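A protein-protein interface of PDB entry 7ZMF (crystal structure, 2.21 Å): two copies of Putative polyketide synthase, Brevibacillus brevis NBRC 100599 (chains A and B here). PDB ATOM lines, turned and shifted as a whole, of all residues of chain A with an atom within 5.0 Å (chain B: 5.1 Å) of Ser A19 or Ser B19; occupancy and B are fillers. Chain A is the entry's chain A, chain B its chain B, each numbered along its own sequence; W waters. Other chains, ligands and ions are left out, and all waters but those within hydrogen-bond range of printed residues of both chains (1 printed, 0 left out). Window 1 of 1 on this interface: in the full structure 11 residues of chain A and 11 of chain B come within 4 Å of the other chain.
The side-chain amide nitrogen (ND2) of Asn A17 sits at hydrogen-bond distance from the backbone carbonyl oxygen (O) of Ser B19 (2.9 Å). The side-chain amide nitrogen (ND2) of Asn B17 sits at hydrogen-bond distance from the backbone carbonyl oxygen (O) of Ser A19 (2.8 Å). NE2 of Gln B24 sits at hydrogen-bond distance from O of Ser A19, at 3.2 Å. O of Asp A20 lies close to OE1 of Gln B24. NE2 of Gln A24 lies within hydrogen-bond range of O of Ser B19 (3.1 Å). OE1 of Gln A24 lies close to O of Asp B20, 3.5 Å away.
The side-chain amide oxygen (OD1) of Asn A17 sits close to the backbone carbonyl oxygen (O) of Arg A25, at 3.1 Å. N of Thr A18 lies within hydrogen-bond range of O of Arg A25 (2.9 Å). OD1 of Asp A20 is in hydrogen-bond range of N of Glu A23 (2.8 Å). The guanidinium group (NH1) of Arg A25 is in salt-bridge range of the side-chain carboxylate (OD2) of Asp A20, 3.2 Å away. OD1 of Asn B17 sits at hydrogen-bond distance from OG of Ser B19, 2.7 Å away. The side-chain carboxylate (OD1) of Asp B20 sits at hydrogen-bond distance from the backbone NH (N) of Glu B23.
Among the printed residues, merely in contact across the chains: Asn A17 with Asn B17 (3.2 Å), Asn A17 with Thr B18 (3.8 Å), Thr A18 with Asn B17 (3.8 Å), Ser A19 with Ser B19 (3.8 Å), Phe A21 with Gln B24 (3.6 Å) and Gln A24 with Phe B21 (3.7 Å).
Of the printed residues of chain B, Thr A18 touches Asn B17. Ser A19 touches three residues of chain B. Of the printed residues of chain B, Gln A24 touches Ser B19 (3.1 Å), Asp B20 (3.3 Å) and Phe B21 (3.7 Å). Printed residues of chain A within 4 Å of Thr B18: Asn A17 (3.8 Å). Of chain A, only Asn A17, Ser A19 and Gln A24 come within 4 Å of Ser B19. Of the printed residues of chain A, Phe B21 touches Gln A24 (3.7 Å). Printed residues of chain A within 4 Å of Gln B24: Ser A19 (3.2 Å), Asp A20 (3.3 Å) and Phe A21 (3.6 Å). Arg B25 touches none of the printed residues of chain A. The nearest printed residue of chain B that does not touch Asp A20 is Asn B17 (4.9 Å).
Printed residues of chain B that touch a printed residue of chain A: Asn B17, Thr B18, Ser B19, Asp B20, Phe B21 and Gln B24. Of the 8 printed residues of chain A, 6 touch a printed residue of chain B. Printed residues of chain A that touch a printed residue of chain B: Asn A17, Thr A18, Ser A19, Asp A20, Phe A21 and Gln A24. Hydrophobic or aromatic side chains of chain A that line the printed part of chain B: Phe A21. Among the printed residues, 12 pairs touch across the chains. Among the printed residues, no Asp or Glu carboxylate lies within 4 Å of a Lys or Arg side-chain nitrogen of the other chain.
Asn A17 touches its own counterpart, Asn B17. Ser B19 touches its own counterpart, Ser A19. Asp A20 touches Gln B24, and with the chains exchanged Gln A24 touches Asp B20. Phe A21 touches Gln B24, and with the chains exchanged Gln A24 touches Phe B21.
Water W1 lies within hydrogen-bond range of N of Asn A17 (2.9 Å) and O of Asn B17 (3.4 Å).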
ATOM      1  N   ASN A  17     -19.801 -33.892 -14.930  1.00  0.00           N
ATOM      2  CA  ASN A  17     -20.250 -32.910 -15.908  1.00  0.00           C
ATOM      3  C   ASN A  17     -19.068 -32.051 -16.339  1.00  0.00           C
ATOM      4  O   ASN A  17     -18.340 -31.514 -15.502  1.00  0.00           O
ATOM      5  CB  ASN A  17     -21.361 -32.061 -15.288  1.00  0.00           C
ATOM      6  CG  ASN A  17     -21.990 -31.099 -16.262  1.00  0.00           C
ATOM      7  OD1 ASN A  17     -21.368 -30.653 -17.228  1.00  0.00           O
ATOM      8  ND2 ASN A  17     -23.236 -30.744 -15.991  1.00  0.00           N
ATOM      9  N   THR A  18     -18.869 -31.934 -17.643  1.00  0.00           N
ATOM     10  CA  THR A  18     -17.776 -31.150 -18.201  1.00  0.00           C
ATOM     11  C   THR A  18     -18.278 -30.171 -19.247  1.00  0.00           C
ATOM     12  O   THR A  18     -17.538 -29.800 -20.169  1.00  0.00           O
ATOM     13  CB  THR A  18     -16.705 -32.059 -18.802  1.00  0.00           C
ATOM     14  OG1 THR A  18     -17.291 -32.883 -19.821  1.00  0.00           O
ATOM     15  CG2 THR A  18     -16.096 -32.956 -17.733  1.00  0.00           C
ATOM     16  N   SER A  19     -19.531 -29.736 -19.123  1.00  0.00           N
ATOM     17  CA  SER A  19     -20.084 -28.807 -20.103  1.00  0.00           C
ATOM     18  C   SER A  19     -19.314 -27.486 -20.125  1.00  0.00           C
ATOM     19  O   SER A  19     -18.737 -27.049 -19.122  1.00  0.00           O
ATOM     20  CB  SER A  19     -21.557 -28.531 -19.806  1.00  0.00           C
ATOM     21  OG  SER A  19     -22.291 -29.735 -19.723  1.00  0.00           O
ATOM     22  N   ASP A  20     -19.318 -26.842 -21.290  1.00  0.00           N
ATOM     23  CA  ASP A  20     -18.740 -25.524 -21.471  1.00  0.00           C
ATOM     24  C   ASP A  20     -19.715 -24.701 -22.300  1.00  0.00           C
ATOM     25  O   ASP A  20     -20.803 -25.173 -22.662  1.00  0.00           O
ATOM     26  CB  ASP A  20     -17.357 -25.606 -22.128  1.00  0.00           C
ATOM     27  CG  ASP A  20     -17.369 -26.376 -23.424  1.00  0.00           C
ATOM     28  OD1 ASP A  20     -18.438 -26.452 -24.073  1.00  0.00           O
ATOM     29  OD2 ASP A  20     -16.306 -26.921 -23.795  1.00  0.00           O
ATOM     30  N   PHE A  21     -19.328 -23.449 -22.589  1.00  0.00           N
ATOM     31  CA  PHE A  21     -20.209 -22.571 -23.347  1.00  0.00           C
ATOM     32  C   PHE A  21     -20.587 -23.171 -24.698  1.00  0.00           C
ATOM     33  O   PHE A  21     -21.630 -22.817 -25.257  1.00  0.00           O
ATOM     34  CB  PHE A  21     -19.550 -21.207 -23.568  1.00  0.00           C
ATOM     35  CG  PHE A  21     -19.552 -20.312 -22.351  1.00  0.00           C
ATOM     36  CD1 PHE A  21     -20.612 -20.318 -21.451  1.00  0.00           C
ATOM     37  CD2 PHE A  21     -18.489 -19.461 -22.112  1.00  0.00           C
ATOM     38  CE1 PHE A  21     -20.606 -19.493 -20.355  1.00  0.00           C
ATOM     39  CE2 PHE A  21     -18.480 -18.634 -21.000  1.00  0.00           C
ATOM     40  CZ  PHE A  21     -19.534 -18.644 -20.140  1.00  0.00           C
ATOM     41  N   GLU A  23     -20.825 -26.707 -25.594  1.00  0.00           N
ATOM     42  CA  GLU A  23     -21.567 -27.955 -25.602  1.00  0.00           C
ATOM     43  C   GLU A  23     -21.911 -28.390 -24.185  1.00  0.00           C
ATOM     44  O   GLU A  23     -21.140 -28.180 -23.251  1.00  0.00           O
ATOM     45  CB  GLU A  23     -20.753 -29.091 -26.266  1.00  0.00           C
ATOM     46  CG  GLU A  23     -20.376 -28.858 -27.722  1.00  0.00           C
ATOM     47  CD  GLU A  23     -18.979 -29.383 -28.052  1.00  0.00           C
ATOM     48  OE1 GLU A  23     -18.361 -30.036 -27.183  1.00  0.00           O
ATOM     49  OE2 GLU A  23     -18.489 -29.129 -29.170  1.00  0.00           O
ATOM     50  N   GLN A  24     -23.080 -29.014 -24.046  1.00  0.00           N
ATOM     51  CA  GLN A  24     -23.360 -29.831 -22.870  1.00  0.00           C
ATOM     52  C   GLN A  24     -22.580 -31.128 -22.995  1.00  0.00           C
ATOM     53  O   GLN A  24     -22.561 -31.747 -24.064  1.00  0.00           O
ATOM     54  CB  GLN A  24     -24.853 -30.111 -22.763  1.00  0.00           C
ATOM     55  CG  GLN A  24     -25.266 -30.885 -21.526  1.00  0.00           C
ATOM     56  CD  GLN A  24     -25.357 -30.002 -20.292  1.00  0.00           C
ATOM     57  OE1 GLN A  24     -25.566 -28.791 -20.399  1.00  0.00           O
ATOM     58  NE2 GLN A  24     -25.201 -30.605 -19.114  1.00  0.00           N
ATOM     59  N   ARG A  25     -21.902 -31.524 -21.923  1.00  0.00           N
ATOM     60  CA  ARG A  25     -20.998 -32.667 -21.994  1.00  0.00           C
ATOM     61  C   ARG A  25     -20.865 -33.338 -20.631  1.00  0.00           C
ATOM     62  O   ARG A  25     -20.896 -32.682 -19.587  1.00  0.00           O
ATOM     63  CB  ARG A  25     -19.613 -32.232 -22.507  1.00  0.00           C
ATOM     64  CG  ARG A  25     -18.613 -33.352 -22.672  1.00  0.00           C
ATOM     65  CD  ARG A  25     -17.213 -32.840 -23.024  1.00  0.00           C
ATOM     66  NE  ARG A  25     -17.185 -31.985 -24.204  1.00  0.00           N
ATOM     67  CZ  ARG A  25     -17.013 -30.668 -24.180  1.00  0.00           C
ATOM     68  NH1 ARG A  25     -16.838 -30.011 -23.042  1.00  0.00           N
ATOM     69  NH2 ARG A  25     -17.009 -29.994 -25.324  1.00  0.00           N
ATOM     70  N   ASN B  17     -18.875 -28.902 -11.810  1.00  0.00           N
ATOM     71  CA  ASN B  17     -19.667 -28.308 -12.875  1.00  0.00           C
ATOM     72  C   ASN B  17     -21.079 -28.885 -12.800  1.00  0.00           C
ATOM     73  O   ASN B  17     -21.249 -30.103 -12.768  1.00  0.00           O
ATOM     74  CB  ASN B  17     -19.027 -28.601 -14.231  1.00  0.00           C
ATOM     75  CG  ASN B  17     -19.733 -27.910 -15.376  1.00  0.00           C
ATOM     76  OD1 ASN B  17     -20.931 -27.614 -15.307  1.00  0.00           O
ATOM     77  ND2 ASN B  17     -18.998 -27.661 -16.452  1.00  0.00           N
ATOM     78  N   THR B  18     -22.085 -28.011 -12.782  1.00  0.00           N
ATOM     79  CA  THR B  18     -23.479 -28.430 -12.701  1.00  0.00           C
ATOM     80  C   THR B  18     -24.305 -27.787 -13.806  1.00  0.00           C
ATOM     81  O   THR B  18     -25.513 -27.593 -13.651  1.00  0.00           O
ATOM     82  CB  THR B  18     -24.070 -28.081 -11.333  1.00  0.00           C
ATOM     83  OG1 THR B  18     -23.988 -26.669 -11.118  1.00  0.00           O
ATOM     84  CG2 THR B  18     -23.323 -28.806 -10.233  1.00  0.00           C
ATOM     85  N   SER B  19     -23.659 -27.444 -14.920  1.00  0.00           N
ATOM     86  CA  SER B  19     -24.348 -26.778 -16.015  1.00  0.00           C
ATOM     87  C   SER B  19     -25.462 -27.665 -16.579  1.00  0.00           C
ATOM     88  O   SER B  19     -25.387 -28.894 -16.545  1.00  0.00           O
ATOM     89  CB  SER B  19     -23.354 -26.446 -17.124  1.00  0.00           C
ATOM     90  OG  SER B  19     -22.254 -25.731 -16.633  1.00  0.00           O
ATOM     91  N   ASP B  20     -26.500 -27.023 -17.112  1.00  0.00           N
ATOM     92  CA  ASP B  20     -27.584 -27.710 -17.797  1.00  0.00           C
ATOM     93  C   ASP B  20     -27.916 -26.948 -19.070  1.00  0.00           C
ATOM     94  O   ASP B  20     -27.268 -25.947 -19.412  1.00  0.00           O
ATOM     95  CB  ASP B  20     -28.807 -27.869 -16.885  1.00  0.00           C
ATOM     96  CG  ASP B  20     -29.281 -26.559 -16.298  1.00  0.00           C
ATOM     97  OD1 ASP B  20     -29.011 -25.503 -16.904  1.00  0.00           O
ATOM     98  OD2 ASP B  20     -29.924 -26.596 -15.214  1.00  0.00           O
ATOM     99  N   PHE B  21     -28.939 -27.434 -19.787  1.00  0.00           N
ATOM    100  CA  PHE B  21     -29.323 -26.815 -21.050  1.00  0.00           C
ATOM    101  C   PHE B  21     -29.651 -25.333 -20.901  1.00  0.00           C
ATOM    102  O   PHE B  21     -29.561 -24.583 -21.881  1.00  0.00           O
ATOM    103  CB  PHE B  21     -30.537 -27.539 -21.649  1.00  0.00           C
ATOM    104  CG  PHE B  21     -30.219 -28.863 -22.289  1.00  0.00           C
ATOM    105  CD1 PHE B  21     -29.033 -29.062 -22.970  1.00  0.00           C
ATOM    106  CD2 PHE B  21     -31.118 -29.915 -22.202  1.00  0.00           C
ATOM    107  CE1 PHE B  21     -28.747 -30.284 -23.551  1.00  0.00           C
ATOM    108  CE2 PHE B  21     -30.838 -31.139 -22.790  1.00  0.00           C
ATOM    109  CZ  PHE B  21     -29.657 -31.323 -23.463  1.00  0.00           C
ATOM    110  N   GLU B  23     -28.396 -22.992 -18.315  1.00  0.00           N
ATOM    111  CA  GLU B  23     -27.347 -22.115 -17.833  1.00  0.00           C
ATOM    112  C   GLU B  23     -26.053 -22.890 -17.635  1.00  0.00           C
ATOM    113  O   GLU B  23     -26.068 -24.073 -17.286  1.00  0.00           O
ATOM    114  CB  GLU B  23     -27.723 -21.450 -16.478  1.00  0.00           C
ATOM    115  CG  GLU B  23     -28.947 -20.559 -16.503  1.00  0.00           C
ATOM    116  CD  GLU B  23     -29.748 -20.658 -15.220  1.00  0.00           C
ATOM    117  OE1 GLU B  23     -29.271 -21.317 -14.268  1.00  0.00           O
ATOM    118  OE2 GLU B  23     -30.851 -20.080 -15.153  1.00  0.00           O
ATOM    119  N   GLN B  24     -24.929 -22.197 -17.849  1.00  0.00           N
ATOM    120  CA  GLN B  24     -23.637 -22.649 -17.348  1.00  0.00           C
ATOM    121  C   GLN B  24     -23.579 -22.387 -15.846  1.00  0.00           C
ATOM    122  O   GLN B  24     -23.952 -21.300 -15.388  1.00  0.00           O
ATOM    123  CB  GLN B  24     -22.511 -21.909 -18.066  1.00  0.00           C
ATOM    124  CG  GLN B  24     -21.115 -22.365 -17.670  1.00  0.00           C
ATOM    125  CD  GLN B  24     -20.679 -23.626 -18.380  1.00  0.00           C
ATOM    126  OE1 GLN B  24     -21.154 -23.929 -19.480  1.00  0.00           O
ATOM    127  NE2 GLN B  24     -19.769 -24.371 -17.762  1.00  0.00           N
ATOM    128  N   ARG B  25     -23.130 -23.384 -15.075  1.00  0.00           N
ATOM    129  CA  ARG B  25     -23.166 -23.271 -13.619  1.00  0.00           C
ATOM    130  C   ARG B  25     -22.069 -24.110 -12.981  1.00  0.00           C
ATOM    131  O   ARG B  25     -21.739 -25.199 -13.461  1.00  0.00           O
ATOM    132  CB  ARG B  25     -24.533 -23.718 -13.056  1.00  0.00           C
ATOM    133  CG  ARG B  25     -24.669 -23.595 -11.559  1.00  0.00           C
ATOM    134  CD  ARG B  25     -25.965 -24.217 -11.035  1.00  0.00           C
ATOM    135  NE  ARG B  25     -27.151 -23.700 -11.702  1.00  0.00           N
ATOM    136  CZ  ARG B  25     -27.879 -24.394 -12.564  1.00  0.00           C
ATOM    137  NH1 ARG B  25     -27.584 -25.652 -12.866  1.00  0.00           N
ATOM    138  NH2 ARG B  25     -28.924 -23.810 -13.145  1.00  0.00           N
HETATM  139  O   HOH W   1     -20.064 -33.251 -12.078  1.00  0.00           O
